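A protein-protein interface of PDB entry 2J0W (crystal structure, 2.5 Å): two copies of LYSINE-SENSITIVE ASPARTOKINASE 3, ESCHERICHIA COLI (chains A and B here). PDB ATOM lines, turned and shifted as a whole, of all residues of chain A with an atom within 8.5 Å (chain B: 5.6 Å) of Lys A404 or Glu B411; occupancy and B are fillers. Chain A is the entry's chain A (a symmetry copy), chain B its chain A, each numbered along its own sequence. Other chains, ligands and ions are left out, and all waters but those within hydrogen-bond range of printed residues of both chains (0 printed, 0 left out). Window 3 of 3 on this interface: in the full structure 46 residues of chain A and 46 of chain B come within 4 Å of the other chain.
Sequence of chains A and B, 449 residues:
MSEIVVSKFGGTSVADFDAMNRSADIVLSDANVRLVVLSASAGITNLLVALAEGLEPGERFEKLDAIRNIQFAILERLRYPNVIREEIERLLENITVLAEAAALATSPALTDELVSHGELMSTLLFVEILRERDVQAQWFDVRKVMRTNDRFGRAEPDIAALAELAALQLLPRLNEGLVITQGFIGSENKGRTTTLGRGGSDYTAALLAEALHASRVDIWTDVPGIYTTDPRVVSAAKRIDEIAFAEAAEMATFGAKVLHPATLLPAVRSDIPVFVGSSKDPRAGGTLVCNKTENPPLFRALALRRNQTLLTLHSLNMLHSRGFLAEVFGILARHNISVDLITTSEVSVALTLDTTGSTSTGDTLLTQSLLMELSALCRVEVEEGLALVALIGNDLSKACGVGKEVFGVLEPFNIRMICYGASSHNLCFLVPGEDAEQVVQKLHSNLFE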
ATOM      1  N   PHE A 299     -12.513  12.971  -1.809  1.00  0.00           N
ATOM      2  CA  PHE A 299     -12.269  11.566  -2.111  1.00  0.00           C
ATOM      3  C   PHE A 299     -11.570  11.436  -3.456  1.00  0.00           C
ATOM      4  O   PHE A 299     -12.190  11.674  -4.490  1.00  0.00           O
ATOM      5  CB  PHE A 299     -13.587  10.787  -2.177  1.00  0.00           C
ATOM      6  CG  PHE A 299     -14.432  10.894  -0.936  1.00  0.00           C
ATOM      7  CD1 PHE A 299     -13.855  10.870   0.327  1.00  0.00           C
ATOM      8  CD2 PHE A 299     -15.819  10.960  -1.034  1.00  0.00           C
ATOM      9  CE1 PHE A 299     -14.638  10.906   1.475  1.00  0.00           C
ATOM     10  CE2 PHE A 299     -16.618  10.994   0.105  1.00  0.00           C
ATOM     11  CZ  PHE A 299     -16.024  10.967   1.367  1.00  0.00           C
ATOM     12  N   ALA A 399     -13.936  16.508   8.507  1.00  0.00           N
ATOM     13  CA  ALA A 399     -15.020  16.734   7.560  1.00  0.00           C
ATOM     14  C   ALA A 399     -16.232  15.933   8.010  1.00  0.00           C
ATOM     15  O   ALA A 399     -16.115  15.095   8.899  1.00  0.00           O
ATOM     16  CB  ALA A 399     -14.593  16.306   6.184  1.00  0.00           C
ATOM     17  N   CYS A 400     -17.386  16.172   7.393  1.00  0.00           N
ATOM     18  CA  CYS A 400     -18.618  15.474   7.778  1.00  0.00           C
ATOM     19  C   CYS A 400     -19.155  14.410   6.828  1.00  0.00           C
ATOM     20  O   CYS A 400     -18.859  14.422   5.634  1.00  0.00           O
ATOM     21  CB  CYS A 400     -19.740  16.487   8.034  1.00  0.00           C
ATOM     22  SG  CYS A 400     -19.549  17.414   9.562  1.00  0.00           S
ATOM     23  N   GLY A 401     -19.948  13.491   7.389  1.00  0.00           N
ATOM     24  CA  GLY A 401     -20.579  12.426   6.623  1.00  0.00           C
ATOM     25  C   GLY A 401     -19.709  11.282   6.140  1.00  0.00           C
ATOM     26  O   GLY A 401     -20.161  10.452   5.347  1.00  0.00           O
ATOM     27  N   VAL A 402     -18.474  11.210   6.623  1.00  0.00           N
ATOM     28  CA  VAL A 402     -17.567  10.161   6.188  1.00  0.00           C
ATOM     29  C   VAL A 402     -18.027   8.745   6.515  1.00  0.00           C
ATOM     30  O   VAL A 402     -17.940   7.860   5.673  1.00  0.00           O
ATOM     31  CB  VAL A 402     -16.158  10.377   6.765  1.00  0.00           C
ATOM     32  CG1 VAL A 402     -15.268   9.183   6.436  1.00  0.00           C
ATOM     33  CG2 VAL A 402     -15.554  11.656   6.191  1.00  0.00           C
ATOM     34  N   GLY A 403     -18.526   8.527   7.723  1.00  0.00           N
ATOM     35  CA  GLY A 403     -18.963   7.190   8.084  1.00  0.00           C
ATOM     36  C   GLY A 403     -20.132   6.642   7.283  1.00  0.00           C
ATOM     37  O   GLY A 403     -20.159   5.459   6.937  1.00  0.00           O
ATOM     38  N   LYS A 404     -21.106   7.498   6.997  1.00  0.00           N
ATOM     39  CA  LYS A 404     -22.298   7.104   6.253  1.00  0.00           C
ATOM     40  C   LYS A 404     -21.949   6.876   4.788  1.00  0.00           C
ATOM     41  O   LYS A 404     -22.364   5.881   4.171  1.00  0.00           O
ATOM     42  CB  LYS A 404     -23.369   8.203   6.377  1.00  0.00           C
ATOM     43  CG  LYS A 404     -24.746   7.894   5.750  1.00  0.00           C
ATOM     44  CD  LYS A 404     -24.793   8.156   4.247  1.00  0.00           C
ATOM     45  CE  LYS A 404     -26.168   7.809   3.682  1.00  0.00           C
ATOM     46  NZ  LYS A 404     -26.265   8.003   2.204  1.00  0.00           N
ATOM     47  N   GLU A 405     -21.164   7.802   4.247  1.00  0.00           N
ATOM     48  CA  GLU A 405     -20.758   7.752   2.854  1.00  0.00           C
ATOM     49  C   GLU A 405     -20.026   6.465   2.480  1.00  0.00           C
ATOM     50  O   GLU A 405     -20.253   5.912   1.403  1.00  0.00           O
ATOM     51  CB  GLU A 405     -19.881   8.963   2.540  1.00  0.00           C
ATOM     52  CG  GLU A 405     -19.897   9.360   1.077  1.00  0.00           C
ATOM     53  CD  GLU A 405     -21.303   9.606   0.558  1.00  0.00           C
ATOM     54  OE1 GLU A 405     -22.073   8.627   0.428  1.00  0.00           O
ATOM     55  OE2 GLU A 405     -21.638  10.779   0.286  1.00  0.00           O
ATOM     56  N   VAL A 406     -19.160   5.988   3.372  1.00  0.00           N
ATOM     57  CA  VAL A 406     -18.383   4.777   3.126  1.00  0.00           C
ATOM     58  C   VAL A 406     -19.090   3.470   3.462  1.00  0.00           C
ATOM     59  O   VAL A 406     -19.024   2.510   2.696  1.00  0.00           O
ATOM     60  CB  VAL A 406     -17.049   4.784   3.922  1.00  0.00           C
ATOM     61  CG1 VAL A 406     -16.451   3.380   3.940  1.00  0.00           C
ATOM     62  CG2 VAL A 406     -16.055   5.753   3.299  1.00  0.00           C
ATOM     63  N   PHE A 407     -19.763   3.432   4.604  1.00  0.00           N
ATOM     64  CA  PHE A 407     -20.420   2.211   5.046  1.00  0.00           C
ATOM     65  C   PHE A 407     -21.906   2.099   4.726  1.00  0.00           C
ATOM     66  O   PHE A 407     -22.574   1.182   5.202  1.00  0.00           O
ATOM     67  CB  PHE A 407     -20.182   2.036   6.549  1.00  0.00           C
ATOM     68  CG  PHE A 407     -18.731   2.125   6.944  1.00  0.00           C
ATOM     69  CD1 PHE A 407     -18.116   3.357   7.131  1.00  0.00           C
ATOM     70  CD2 PHE A 407     -17.969   0.979   7.076  1.00  0.00           C
ATOM     71  CE1 PHE A 407     -16.761   3.440   7.441  1.00  0.00           C
ATOM     72  CE2 PHE A 407     -16.613   1.051   7.385  1.00  0.00           C
ATOM     73  CZ  PHE A 407     -16.008   2.282   7.568  1.00  0.00           C
ATOM     74  N   GLY A 408     -22.416   3.019   3.910  1.00  0.00           N
ATOM     75  CA  GLY A 408     -23.822   2.982   3.547  1.00  0.00           C
ATOM     76  C   GLY A 408     -24.126   1.871   2.557  1.00  0.00           C
ATOM     77  O   GLY A 408     -25.240   1.333   2.513  1.00  0.00           O
ATOM     78  N   VAL A 409     -23.111   1.511   1.777  1.00  0.00           N
ATOM     79  CA  VAL A 409     -23.233   0.480   0.753  1.00  0.00           C
ATOM     80  C   VAL A 409     -22.772  -0.910   1.182  1.00  0.00           C
ATOM     81  O   VAL A 409     -23.136  -1.914   0.564  1.00  0.00           O
ATOM     82  CB  VAL A 409     -22.404   0.856  -0.476  1.00  0.00           C
ATOM     83  CG1 VAL A 409     -22.857   0.045  -1.671  1.00  0.00           C
ATOM     84  CG2 VAL A 409     -22.512   2.344  -0.735  1.00  0.00           C
ATOM     85  N   LEU A 410     -21.977  -0.964   2.244  1.00  0.00           N
ATOM     86  CA  LEU A 410     -21.405  -2.212   2.738  1.00  0.00           C
ATOM     87  C   LEU A 410     -22.247  -2.995   3.726  1.00  0.00           C
ATOM     88  O   LEU A 410     -21.743  -3.897   4.391  1.00  0.00           O
ATOM     89  CB  LEU A 410     -20.045  -1.901   3.353  1.00  0.00           C
ATOM     90  CG  LEU A 410     -19.303  -0.889   2.472  1.00  0.00           C
ATOM     91  CD1 LEU A 410     -17.995  -0.467   3.107  1.00  0.00           C
ATOM     92  CD2 LEU A 410     -19.068  -1.506   1.111  1.00  0.00           C
ATOM     93  N   LEU A 427      -8.789   6.367   5.156  1.00  0.00           N
ATOM     94  CA  LEU A 427      -9.657   5.592   6.022  1.00  0.00           C
ATOM     95  C   LEU A 427      -9.610   4.173   5.473  1.00  0.00           C
ATOM     96  O   LEU A 427     -10.093   3.917   4.367  1.00  0.00           O
ATOM     97  CB  LEU A 427     -11.087   6.116   5.963  1.00  0.00           C
ATOM     98  CG  LEU A 427     -12.067   5.413   6.906  1.00  0.00           C
ATOM     99  CD1 LEU A 427     -13.240   6.334   7.156  1.00  0.00           C
ATOM    100  CD2 LEU A 427     -12.531   4.076   6.333  1.00  0.00           C
ATOM    101  N   LEU A 443     -18.423   0.937  -3.558  1.00  0.00           N
ATOM    102  CA  LEU A 443     -17.983   2.250  -3.075  1.00  0.00           C
ATOM    103  C   LEU A 443     -17.787   3.242  -4.205  1.00  0.00           C
ATOM    104  O   LEU A 443     -18.454   4.271  -4.284  1.00  0.00           O
ATOM    105  CB  LEU A 443     -16.661   2.136  -2.321  1.00  0.00           C
ATOM    106  CG  LEU A 443     -16.606   1.369  -1.006  1.00  0.00           C
ATOM    107  CD1 LEU A 443     -15.181   1.432  -0.499  1.00  0.00           C
ATOM    108  CD2 LEU A 443     -17.559   1.972   0.011  1.00  0.00           C
ATOM    109  N   ASN A 446     -21.172   4.839  -5.973  1.00  0.00           N
ATOM    110  CA  ASN A 446     -21.839   5.980  -5.369  1.00  0.00           C
ATOM    111  C   ASN A 446     -20.755   6.881  -4.781  1.00  0.00           C
ATOM    112  O   ASN A 446     -20.937   7.458  -3.709  1.00  0.00           O
ATOM    113  CB  ASN A 446     -22.822   5.535  -4.262  1.00  0.00           C
ATOM    114  CG  ASN A 446     -22.133   5.270  -2.945  1.00  0.00           C
ATOM    115  OD1 ASN A 446     -21.266   4.409  -2.877  1.00  0.00           O
ATOM    116  ND2 ASN A 446     -22.497   6.017  -1.898  1.00  0.00           N
ATOM    117  N   PHE B 407     -23.133   3.970  11.398  1.00  0.00           N
ATOM    118  CA  PHE B 407     -22.902   5.247  10.741  1.00  0.00           C
ATOM    119  C   PHE B 407     -23.980   5.699   9.763  1.00  0.00           C
ATOM    120  O   PHE B 407     -23.791   6.680   9.044  1.00  0.00           O
ATOM    121  CB  PHE B 407     -21.534   5.210  10.051  1.00  0.00           C
ATOM    122  CG  PHE B 407     -20.412   4.780  10.959  1.00  0.00           C
ATOM    123  CD1 PHE B 407     -20.169   3.434  11.206  1.00  0.00           C
ATOM    124  CD2 PHE B 407     -19.635   5.722  11.606  1.00  0.00           C
ATOM    125  CE1 PHE B 407     -19.168   3.039  12.089  1.00  0.00           C
ATOM    126  CE2 PHE B 407     -18.632   5.337  12.492  1.00  0.00           C
ATOM    127  CZ  PHE B 407     -18.397   3.995  12.734  1.00  0.00           C
ATOM    128  N   GLY B 408     -25.110   4.997   9.747  1.00  0.00           N
ATOM    129  CA  GLY B 408     -26.192   5.363   8.851  1.00  0.00           C
ATOM    130  C   GLY B 408     -26.921   6.611   9.318  1.00  0.00           C
ATOM    131  O   GLY B 408     -27.480   7.371   8.515  1.00  0.00           O
ATOM    132  N   VAL B 409     -26.888   6.832  10.629  1.00  0.00           N
ATOM    133  CA  VAL B 409     -27.557   7.968  11.252  1.00  0.00           C
ATOM    134  C   VAL B 409     -26.664   9.179  11.509  1.00  0.00           C
ATOM    135  O   VAL B 409     -27.154  10.296  11.694  1.00  0.00           O
ATOM    136  CB  VAL B 409     -28.140   7.560  12.605  1.00  0.00           C
ATOM    137  CG1 VAL B 409     -29.179   8.568  13.045  1.00  0.00           C
ATOM    138  CG2 VAL B 409     -28.717   6.162  12.517  1.00  0.00           C
ATOM    139  N   LEU B 410     -25.356   8.954  11.512  1.00  0.00           N
ATOM    140  CA  LEU B 410     -24.378   9.996  11.803  1.00  0.00           C
ATOM    141  C   LEU B 410     -23.909  10.829  10.626  1.00  0.00           C
ATOM    142  O   LEU B 410     -22.906  11.531  10.724  1.00  0.00           O
ATOM    143  CB  LEU B 410     -23.179   9.347  12.483  1.00  0.00           C
ATOM    144  CG  LEU B 410     -23.666   8.300  13.493  1.00  0.00           C
ATOM    145  CD1 LEU B 410     -22.504   7.551  14.109  1.00  0.00           C
ATOM    146  CD2 LEU B 410     -24.486   8.995  14.559  1.00  0.00           C
ATOM    147  N   GLU B 411     -24.640  10.756   9.519  1.00  0.00           N
ATOM    148  CA  GLU B 411     -24.284  11.502   8.315  1.00  0.00           C
ATOM    149  C   GLU B 411     -23.991  12.960   8.618  1.00  0.00           C
ATOM    150  O   GLU B 411     -22.967  13.495   8.198  1.00  0.00           O
ATOM    151  CB  GLU B 411     -25.402  11.412   7.276  1.00  0.00           C
ATOM    152  CG  GLU B 411     -25.260  12.401   6.129  1.00  0.00           C
ATOM    153  CD  GLU B 411     -26.349  12.249   5.095  1.00  0.00           C
ATOM    154  OE1 GLU B 411     -27.433  11.729   5.444  1.00  0.00           O
ATOM    155  OE2 GLU B 411     -26.125  12.663   3.940  1.00  0.00           O
ATOM    156  N   PRO B 412     -24.890  13.621   9.355  1.00  0.00           N
ATOM    157  CA  PRO B 412     -24.735  15.031   9.721  1.00  0.00           C
ATOM    158  C   PRO B 412     -23.569  15.386  10.662  1.00  0.00           C
ATOM    159  O   PRO B 412     -23.393  16.557  11.011  1.00  0.00           O
ATOM    160  CB  PRO B 412     -26.093  15.361  10.340  1.00  0.00           C
ATOM    161  CG  PRO B 412     -26.497  14.051  10.965  1.00  0.00           C
ATOM    162  CD  PRO B 412     -26.170  13.089   9.860  1.00  0.00           C
ATOM    163  N   PHE B 413     -22.768  14.395  11.051  1.00  0.00           N
ATOM    164  CA  PHE B 413     -21.668  14.642  11.982  1.00  0.00           C
ATOM    165  C   PHE B 413     -20.238  14.436  11.501  1.00  0.00           C
ATOM    166  O   PHE B 413     -19.990  13.946  10.403  1.00  0.00           O
ATOM    167  CB  PHE B 413     -21.867  13.797  13.233  1.00  0.00           C
ATOM    168  CG  PHE B 413     -23.206  13.967  13.866  1.00  0.00           C
ATOM    169  CD1 PHE B 413     -24.053  12.875  14.019  1.00  0.00           C
ATOM    170  CD2 PHE B 413     -23.619  15.211  14.329  1.00  0.00           C
ATOM    171  CE1 PHE B 413     -25.296  13.015  14.626  1.00  0.00           C
ATOM    172  CE2 PHE B 413     -24.861  15.362  14.938  1.00  0.00           C
ATOM    173  CZ  PHE B 413     -25.702  14.256  15.087  1.00  0.00           C
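The backbone NH of Gly A401 lies close to the backbone carbonyl oxygen of Glu B411 (3.1 Å).
The backbone NH of Lys A404 lies close to the backbone carbonyl oxygen of Phe B407, at 3.5 Å.
N of Gly A401 lies within hydrogen-bond range of O of Phe B413 (3.0 Å).
The side-chain sulfur (SG) of Cys A400 sits close to the backbone carbonyl oxygen (O) of Phe B413, at 3.6 Å.
Among the printed residues, merely in contact across the chains: Gly A403 with Phe B407 (3.4 Å), Lys A404 with Glu B411 (3.9 Å) and Lys A404 with Gly B408 (3.9 Å).
Of chain B, only Phe B407, Gly B408 and Glu B411 come within 4 Å of Lys A404.
Of chain A, only Gly A401 (3.1 Å) and Lys A404 (3.9 Å) come within 4 Å of Glu B411.
No residue of chain A comes within 4 Å of Pro B412.
Printed residues of chain A within 4 Å of Phe B407: Gly A403 and Lys A404.
Printed residues of chain B within 4 Å of Cys A400: Phe B413 (3.3 Å).
Printed residues of chain B within 4 Å of Gly A401: Glu B411 and Phe B413.
Of the printed residues of chain A, Gly B408 touches Lys A404 (3.9 Å).
Leu A410 touches none of the printed residues of chain B.
Val A406 touches none of the printed residues of chain B.
The nearest printed residue of chain B that does not touch Gly A401 is Leu B410 (4.8 Å).
Of the 16 printed residues of chain A, 4 touch a printed residue of chain B.
Along chain A the printed residues that touch a printed residue of chain B span positions 400 to 404.
Of the 7 printed residues of chain B, 4 touch a printed residue of chain A.
Hydrophobic or aromatic side chains of chain B that line the printed part of chain A: Phe B407.
Positions printed for both chains: 407, 408, 409 and 410.
Of the 7 pairs that touch across the chains among the printed residues, none has its exchanged pair printed and touching as well.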
